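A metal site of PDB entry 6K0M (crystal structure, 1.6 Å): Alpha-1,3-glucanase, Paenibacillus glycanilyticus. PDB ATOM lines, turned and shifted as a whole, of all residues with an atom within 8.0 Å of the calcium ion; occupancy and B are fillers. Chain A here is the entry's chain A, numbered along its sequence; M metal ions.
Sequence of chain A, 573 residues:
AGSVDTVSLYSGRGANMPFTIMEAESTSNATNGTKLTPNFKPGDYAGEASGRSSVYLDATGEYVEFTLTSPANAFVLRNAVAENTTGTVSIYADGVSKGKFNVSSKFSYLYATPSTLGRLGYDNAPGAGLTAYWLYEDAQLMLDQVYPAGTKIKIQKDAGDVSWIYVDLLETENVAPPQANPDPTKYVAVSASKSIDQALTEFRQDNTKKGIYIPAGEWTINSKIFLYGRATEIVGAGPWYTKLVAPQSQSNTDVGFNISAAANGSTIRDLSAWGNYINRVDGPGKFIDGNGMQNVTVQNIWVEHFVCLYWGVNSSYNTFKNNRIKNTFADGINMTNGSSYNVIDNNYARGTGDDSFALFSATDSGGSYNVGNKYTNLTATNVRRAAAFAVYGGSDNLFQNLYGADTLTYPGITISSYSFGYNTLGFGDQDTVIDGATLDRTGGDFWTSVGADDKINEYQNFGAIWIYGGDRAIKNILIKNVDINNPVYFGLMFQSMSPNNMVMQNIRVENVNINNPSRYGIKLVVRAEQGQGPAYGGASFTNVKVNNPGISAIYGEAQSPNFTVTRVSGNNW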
ATOM      1  N   ILE A  21      10.794  -3.287  -8.588  1.00  0.00           N
ATOM      2  CA  ILE A  21      11.652  -2.550  -7.661  1.00  0.00           C
ATOM      3  C   ILE A  21      11.941  -3.448  -6.465  1.00  0.00           C
ATOM      4  O   ILE A  21      11.016  -3.890  -5.774  1.00  0.00           O
ATOM      5  CB  ILE A  21      10.975  -1.245  -7.187  1.00  0.00           C
ATOM      6  CG1 ILE A  21      10.628  -0.336  -8.382  1.00  0.00           C
ATOM      7  CG2 ILE A  21      11.860  -0.544  -6.141  1.00  0.00           C
ATOM      8  CD1 ILE A  21      11.765   0.550  -8.834  1.00  0.00           C
ATOM      9  N   MET A  22      13.218  -3.697  -6.198  1.00  0.00           N
ATOM     10  CA  MET A  22      13.605  -4.563  -5.077  1.00  0.00           C
ATOM     11  C   MET A  22      14.551  -3.817  -4.142  1.00  0.00           C
ATOM     12  O   MET A  22      15.584  -3.304  -4.570  1.00  0.00           O
ATOM     13  CB  MET A  22      14.228  -5.853  -5.605  1.00  0.00           C
ATOM     14  CG  MET A  22      13.220  -6.676  -6.431  1.00  0.00           C
ATOM     15  SD  MET A  22      13.682  -8.406  -6.457  1.00  0.00           S
ATOM     16  CE  MET A  22      15.208  -8.220  -7.338  1.00  0.00           C
ATOM     17  N   GLU A  23      14.173  -3.728  -2.862  1.00  0.00           N
ATOM     18  CA  GLU A  23      15.008  -3.013  -1.892  1.00  0.00           C
ATOM     19  C   GLU A  23      16.195  -3.869  -1.492  1.00  0.00           C
ATOM     20  O   GLU A  23      16.053  -5.053  -1.188  1.00  0.00           O
ATOM     21  CB  GLU A  23      14.199  -2.638  -0.652  1.00  0.00           C
ATOM     22  CG  GLU A  23      13.038  -1.674  -0.906  1.00  0.00           C
ATOM     23  CD  GLU A  23      13.481  -0.270  -1.265  1.00  0.00           C
ATOM     24  OE1 GLU A  23      14.691   0.041  -1.218  1.00  0.00           O
ATOM     25  OE2 GLU A  23      12.587   0.535  -1.608  1.00  0.00           O
ATOM     26  N   ALA A  24      17.367  -3.241  -1.452  1.00  0.00           N
ATOM     27  CA  ALA A  24      18.572  -3.980  -1.096  1.00  0.00           C
ATOM     28  C   ALA A  24      18.475  -4.533   0.319  1.00  0.00           C
ATOM     29  O   ALA A  24      18.893  -5.673   0.579  1.00  0.00           O
ATOM     30  CB  ALA A  24      19.796  -3.074  -1.225  1.00  0.00           C
ATOM     31  N   GLU A  25      17.895  -3.762   1.233  1.00  0.00           N
ATOM     32  CA  GLU A  25      17.873  -4.086   2.646  1.00  0.00           C
ATOM     33  C   GLU A  25      16.827  -5.115   3.017  1.00  0.00           C
ATOM     34  O   GLU A  25      16.686  -5.420   4.211  1.00  0.00           O
ATOM     35  CB  GLU A  25      17.654  -2.793   3.455  1.00  0.00           C
ATOM     36  CG  GLU A  25      16.298  -2.129   3.208  1.00  0.00           C
ATOM     37  CD  GLU A  25      16.308  -1.148   2.035  1.00  0.00           C
ATOM     38  OE1 GLU A  25      17.225  -1.207   1.176  1.00  0.00           O
ATOM     39  OE2 GLU A  25      15.398  -0.312   1.974  1.00  0.00           O
ATOM     40  N   SER A  26      16.086  -5.658   2.054  1.00  0.00           N
ATOM     41  CA  SER A  26      15.090  -6.671   2.356  1.00  0.00           C
ATOM     42  C   SER A  26      15.705  -7.813   3.161  1.00  0.00           C
ATOM     43  O   SER A  26      16.828  -8.237   2.895  1.00  0.00           O
ATOM     44  CB  SER A  26      14.486  -7.223   1.064  1.00  0.00           C
ATOM     45  OG  SER A  26      13.669  -8.350   1.350  1.00  0.00           O
ATOM     46  N   TYR A  45      22.426   9.144   4.280  1.00  0.00           N
ATOM     47  CA  TYR A  45      22.351   8.002   3.368  1.00  0.00           C
ATOM     48  C   TYR A  45      21.174   7.087   3.668  1.00  0.00           C
ATOM     49  O   TYR A  45      20.702   6.370   2.778  1.00  0.00           O
ATOM     50  CB  TYR A  45      23.666   7.219   3.379  1.00  0.00           C
ATOM     51  CG  TYR A  45      24.796   7.972   2.718  1.00  0.00           C
ATOM     52  CD1 TYR A  45      24.815   8.194   1.342  1.00  0.00           C
ATOM     53  CD2 TYR A  45      25.825   8.504   3.485  1.00  0.00           C
ATOM     54  CE1 TYR A  45      25.845   8.913   0.746  1.00  0.00           C
ATOM     55  CE2 TYR A  45      26.848   9.222   2.902  1.00  0.00           C
ATOM     56  CZ  TYR A  45      26.855   9.420   1.534  1.00  0.00           C
ATOM     57  OH  TYR A  45      27.876  10.143   0.982  1.00  0.00           O
ATOM     58  N   ALA A  46      20.702   7.053   4.918  1.00  0.00           N
ATOM     59  CA  ALA A  46      19.459   6.323   5.177  1.00  0.00           C
ATOM     60  C   ALA A  46      18.244   7.185   4.866  1.00  0.00           C
ATOM     61  O   ALA A  46      17.343   6.746   4.140  1.00  0.00           O
ATOM     62  CB  ALA A  46      19.408   5.847   6.636  1.00  0.00           C
ATOM     63  N   GLU A  48      17.668   9.459   2.842  1.00  0.00           N
ATOM     64  CA  GLU A  48      17.426   9.714   1.426  1.00  0.00           C
ATOM     65  C   GLU A  48      17.245   8.446   0.615  1.00  0.00           C
ATOM     66  O   GLU A  48      16.984   8.538  -0.596  1.00  0.00           O
ATOM     67  CB  GLU A  48      18.559  10.551   0.817  1.00  0.00           C
ATOM     68  CG  GLU A  48      18.580  11.984   1.341  1.00  0.00           C
ATOM     69  CD  GLU A  48      19.354  12.930   0.453  1.00  0.00           C
ATOM     70  OE1 GLU A  48      19.765  12.509  -0.645  1.00  0.00           O
ATOM     71  OE2 GLU A  48      19.528  14.105   0.855  1.00  0.00           O
ATOM     72  N   ALA A  49      17.380   7.281   1.226  1.00  0.00           N
ATOM     73  CA  ALA A  49      17.232   6.020   0.522  1.00  0.00           C
ATOM     74  C   ALA A  49      15.765   5.646   0.364  1.00  0.00           C
ATOM     75  O   ALA A  49      14.915   6.000   1.185  1.00  0.00           O
ATOM     76  CB  ALA A  49      17.941   4.900   1.266  1.00  0.00           C
ATOM     77  N   SER A  50      15.479   4.906  -0.715  1.00  0.00           N
ATOM     78  CA  SER A  50      14.173   4.254  -0.821  1.00  0.00           C
ATOM     79  C   SER A  50      14.004   3.280   0.337  1.00  0.00           C
ATOM     80  O   SER A  50      14.926   2.540   0.689  1.00  0.00           O
ATOM     81  CB  SER A  50      14.086   3.535  -2.176  1.00  0.00           C
ATOM     82  OG  SER A  50      12.826   2.893  -2.370  1.00  0.00           O
ATOM     83  N   GLY A  51      12.848   3.329   0.982  1.00  0.00           N
ATOM     84  CA  GLY A  51      12.652   2.549   2.194  1.00  0.00           C
ATOM     85  C   GLY A  51      13.379   3.076   3.408  1.00  0.00           C
ATOM     86  O   GLY A  51      13.336   2.427   4.464  1.00  0.00           O
ATOM     87  N   ARG A  52      14.053   4.221   3.270  1.00  0.00           N
ATOM     88  CA  ARG A  52      14.886   4.830   4.310  1.00  0.00           C
ATOM     89  C   ARG A  52      16.018   3.909   4.751  1.00  0.00           C
ATOM     90  O   ARG A  52      16.501   4.005   5.870  1.00  0.00           O
ATOM     91  CB  ARG A  52      14.047   5.274   5.518  1.00  0.00           C
ATOM     92  CG  ARG A  52      12.849   6.151   5.137  1.00  0.00           C
ATOM     93  CD  ARG A  52      13.244   7.461   4.442  1.00  0.00           C
ATOM     94  NE  ARG A  52      12.030   8.198   4.089  1.00  0.00           N
ATOM     95  CZ  ARG A  52      11.889   9.524   4.117  1.00  0.00           C
ATOM     96  NH1 ARG A  52      12.908  10.319   4.438  1.00  0.00           N
ATOM     97  NH2 ARG A  52      10.710  10.066   3.804  1.00  0.00           N
ATOM     98  N   SER A  53      16.474   3.024   3.855  1.00  0.00           N
ATOM     99  CA  SER A  53      17.622   2.198   4.194  1.00  0.00           C
ATOM    100  C   SER A  53      18.309   1.742   2.908  1.00  0.00           C
ATOM    101  O   SER A  53      17.714   1.699   1.825  1.00  0.00           O
ATOM    102  CB  SER A  53      17.202   0.990   5.038  1.00  0.00           C
ATOM    103  OG  SER A  53      18.317   0.149   5.293  1.00  0.00           O
ATOM    104  N   SER A  54      19.592   1.423   3.064  1.00  0.00           N
ATOM    105  CA  SER A  54      20.380   0.825   2.002  1.00  0.00           C
ATOM    106  C   SER A  54      21.393  -0.102   2.644  1.00  0.00           C
ATOM    107  O   SER A  54      21.528  -0.159   3.867  1.00  0.00           O
ATOM    108  CB  SER A  54      21.061   1.906   1.147  1.00  0.00           C
ATOM    109  OG  SER A  54      21.906   2.720   1.930  1.00  0.00           O
ATOM    110  N   VAL A  55      22.101  -0.848   1.810  1.00  0.00           N
ATOM    111  CA  VAL A  55      23.169  -1.731   2.289  1.00  0.00           C
ATOM    112  C   VAL A  55      24.493  -1.149   1.814  1.00  0.00           C
ATOM    113  O   VAL A  55      24.719  -0.955   0.616  1.00  0.00           O
ATOM    114  CB  VAL A  55      23.004  -3.184   1.807  1.00  0.00           C
ATOM    115  CG1 VAL A  55      24.160  -4.037   2.352  1.00  0.00           C
ATOM    116  CG2 VAL A  55      21.686  -3.759   2.310  1.00  0.00           C
ATOM    117  N   PHE A  66      20.275 -10.265  -4.296  1.00  0.00           N
ATOM    118  CA  PHE A  66      18.861 -10.206  -4.651  1.00  0.00           C
ATOM    119  C   PHE A  66      18.428 -11.529  -5.281  1.00  0.00           C
ATOM    120  O   PHE A  66      19.242 -12.292  -5.798  1.00  0.00           O
ATOM    121  CB  PHE A  66      18.580  -9.080  -5.652  1.00  0.00           C
ATOM    122  CG  PHE A  66      18.929  -7.705  -5.174  1.00  0.00           C
ATOM    123  CD1 PHE A  66      20.240  -7.223  -5.270  1.00  0.00           C
ATOM    124  CD2 PHE A  66      17.956  -6.858  -4.671  1.00  0.00           C
ATOM    125  CE1 PHE A  66      20.556  -5.955  -4.853  1.00  0.00           C
ATOM    126  CE2 PHE A  66      18.269  -5.580  -4.255  1.00  0.00           C
ATOM    127  CZ  PHE A  66      19.576  -5.123  -4.354  1.00  0.00           C
ATOM    128  N   ARG A  78      20.147   1.831  -7.943  1.00  0.00           N
ATOM    129  CA  ARG A  78      20.184   3.107  -7.236  1.00  0.00           C
ATOM    130  C   ARG A  78      21.203   3.001  -6.114  1.00  0.00           C
ATOM    131  O   ARG A  78      21.150   2.073  -5.304  1.00  0.00           O
ATOM    132  CB  ARG A  78      18.812   3.507  -6.680  1.00  0.00           C
ATOM    133  CG  ARG A  78      18.775   4.952  -6.156  1.00  0.00           C
ATOM    134  CD  ARG A  78      17.375   5.353  -5.720  1.00  0.00           C
ATOM    135  NE  ARG A  78      17.184   6.805  -5.670  1.00  0.00           N
ATOM    136  CZ  ARG A  78      17.075   7.524  -4.552  1.00  0.00           C
ATOM    137  NH1 ARG A  78      17.165   6.956  -3.348  1.00  0.00           N
ATOM    138  NH2 ARG A  78      16.862   8.827  -4.638  1.00  0.00           N
ATOM    139  N   TYR A 136      21.895  10.119  -3.802  1.00  0.00           N
ATOM    140  CA  TYR A 136      21.754   8.889  -4.591  1.00  0.00           C
ATOM    141  C   TYR A 136      21.669   9.196  -6.080  1.00  0.00           C
ATOM    142  O   TYR A 136      21.232  10.273  -6.488  1.00  0.00           O
ATOM    143  CB  TYR A 136      20.517   8.118  -4.143  1.00  0.00           C
ATOM    144  CG  TYR A 136      20.783   7.380  -2.844  1.00  0.00           C
ATOM    145  CD1 TYR A 136      21.375   6.123  -2.863  1.00  0.00           C
ATOM    146  CD2 TYR A 136      20.519   7.970  -1.613  1.00  0.00           C
ATOM    147  CE1 TYR A 136      21.669   5.448  -1.693  1.00  0.00           C
ATOM    148  CE2 TYR A 136      20.794   7.301  -0.429  1.00  0.00           C
ATOM    149  CZ  TYR A 136      21.373   6.044  -0.488  1.00  0.00           C
ATOM    150  OH  TYR A 136      21.676   5.371   0.679  1.00  0.00           O
ATOM    151  N   VAL A 167      24.087   0.604  -1.606  1.00  0.00           N
ATOM    152  CA  VAL A 167      23.169  -0.047  -2.540  1.00  0.00           C
ATOM    153  C   VAL A 167      21.762   0.125  -1.991  1.00  0.00           C
ATOM    154  O   VAL A 167      21.417  -0.435  -0.948  1.00  0.00           O
ATOM    155  CB  VAL A 167      23.525  -1.522  -2.742  1.00  0.00           C
ATOM    156  CG1 VAL A 167      22.540  -2.170  -3.714  1.00  0.00           C
ATOM    157  CG2 VAL A 167      24.962  -1.665  -3.242  1.00  0.00           C
ATOM    158  N   ASP A 168      20.925   0.885  -2.709  1.00  0.00           N
ATOM    159  CA  ASP A 168      19.614   1.256  -2.192  1.00  0.00           C
ATOM    160  C   ASP A 168      18.521   0.318  -2.703  1.00  0.00           C
ATOM    161  O   ASP A 168      17.793  -0.287  -1.913  1.00  0.00           O
ATOM    162  CB  ASP A 168      19.311   2.711  -2.592  1.00  0.00           C
ATOM    163  CG  ASP A 168      17.977   3.189  -2.086  1.00  0.00           C
ATOM    164  OD1 ASP A 168      17.340   2.481  -1.272  1.00  0.00           O
ATOM    165  OD2 ASP A 168      17.540   4.285  -2.510  1.00  0.00           O
ATOM    166  N   LEU A 169      18.419   0.188  -4.024  1.00  0.00           N
ATOM    167  CA  LEU A 169      17.431  -0.688  -4.629  1.00  0.00           C
ATOM    168  C   LEU A 169      17.965  -1.131  -5.975  1.00  0.00           C
ATOM    169  O   LEU A 169      18.916  -0.568  -6.512  1.00  0.00           O
ATOM    170  CB  LEU A 169      16.075   0.002  -4.786  1.00  0.00           C
ATOM    171  CG  LEU A 169      15.989   1.243  -5.684  1.00  0.00           C
ATOM    172  CD1 LEU A 169      15.896   0.883  -7.182  1.00  0.00           C
ATOM    173  CD2 LEU A 169      14.772   2.081  -5.309  1.00  0.00           C
ATOM    174  N   LEU A 170      17.309  -2.151  -6.519  1.00  0.00           N
ATOM    175  CA  LEU A 170      17.587  -2.679  -7.855  1.00  0.00           C
ATOM    176  C   LEU A 170      16.280  -2.728  -8.622  1.00  0.00           C
ATOM    177  O   LEU A 170      15.312  -3.338  -8.143  1.00  0.00           O
ATOM    178  CB  LEU A 170      18.201  -4.068  -7.750  1.00  0.00           C
ATOM    179  CG  LEU A 170      18.632  -4.740  -9.045  1.00  0.00           C
ATOM    180  CD1 LEU A 170      19.873  -4.046  -9.580  1.00  0.00           C
ATOM    181  CD2 LEU A 170      18.899  -6.219  -8.778  1.00  0.00           C
ATOM    182  N   ASN A 382      10.847   8.783  -3.723  1.00  0.00           N
ATOM    183  CA  ASN A 382      12.114   9.494  -3.516  1.00  0.00           C
ATOM    184  C   ASN A 382      12.011  10.936  -4.015  1.00  0.00           C
ATOM    185  O   ASN A 382      12.801  11.394  -4.846  1.00  0.00           O
ATOM    186  CB  ASN A 382      13.279   8.769  -4.193  1.00  0.00           C
ATOM    187  CG  ASN A 382      13.636   7.488  -3.501  1.00  0.00           C
ATOM    188  OD1 ASN A 382      13.599   6.412  -4.100  1.00  0.00           O
ATOM    189  ND2 ASN A 382      14.023   7.589  -2.233  1.00  0.00           N
ATOM    190  N   ASP A 406       8.515   8.189   0.399  1.00  0.00           N
ATOM    191  CA  ASP A 406       9.857   8.675   0.708  1.00  0.00           C
ATOM    192  C   ASP A 406      10.077  10.104   0.185  1.00  0.00           C
ATOM    193  O   ASP A 406      10.960  10.374  -0.621  1.00  0.00           O
ATOM    194  CB  ASP A 406      10.904   7.689   0.179  1.00  0.00           C
ATOM    195  CG  ASP A 406      10.876   6.386   0.940  1.00  0.00           C
ATOM    196  OD1 ASP A 406      10.792   6.441   2.188  1.00  0.00           O
ATOM    197  OD2 ASP A 406      10.929   5.303   0.310  1.00  0.00           O
ATOM    198  N   ARG A 441       5.819   6.536   4.242  1.00  0.00           N
ATOM    199  CA  ARG A 441       6.908   7.366   4.749  1.00  0.00           C
ATOM    200  C   ARG A 441       6.948   8.737   4.053  1.00  0.00           C
ATOM    201  O   ARG A 441       7.981   9.187   3.567  1.00  0.00           O
ATOM    202  CB  ARG A 441       8.256   6.632   4.602  1.00  0.00           C
ATOM    203  CG  ARG A 441       8.295   5.289   5.367  1.00  0.00           C
ATOM    204  CD  ARG A 441       9.540   4.439   4.999  1.00  0.00           C
ATOM    205  NE  ARG A 441       9.653   4.254   3.554  1.00  0.00           N
ATOM    206  CZ  ARG A 441       9.009   3.317   2.847  1.00  0.00           C
ATOM    207  NH1 ARG A 441       8.240   2.422   3.455  1.00  0.00           N
ATOM    208  NH2 ARG A 441       9.158   3.263   1.530  1.00  0.00           N
HETATM  209 CA    CA M   1      16.457   0.851   0.028  1.00  0.00          CA
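The calcium ion is bound by OD1 of Asp 168 (2.3 Å), OE1 of Glu 23 (2.3 Å), O of Ser 53 (2.4 Å), O of Ser 50 (2.4 Å), OE1 of Glu 25 (2.5 Å), OE2 of Glu 25 (2.5 Å) and O of Asp 168 (2.6 Å). The calcium ion has seven donor atoms within binding distance.
The backbone NH (N) of Ala 24 sits close to the backbone carbonyl oxygen (O) of Asp 168. The side-chain amide nitrogen (ND2) of Asn 382 sits close to the backbone NH (N) of Ser 50, 3.4 Å away. OD2 of Asp 168 lies within salt-bridge range of NH1 of Arg 78 (2.8 Å).
The nearest printed residue that does not touch the calcium ion is Ser 54 (4.4 Å).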
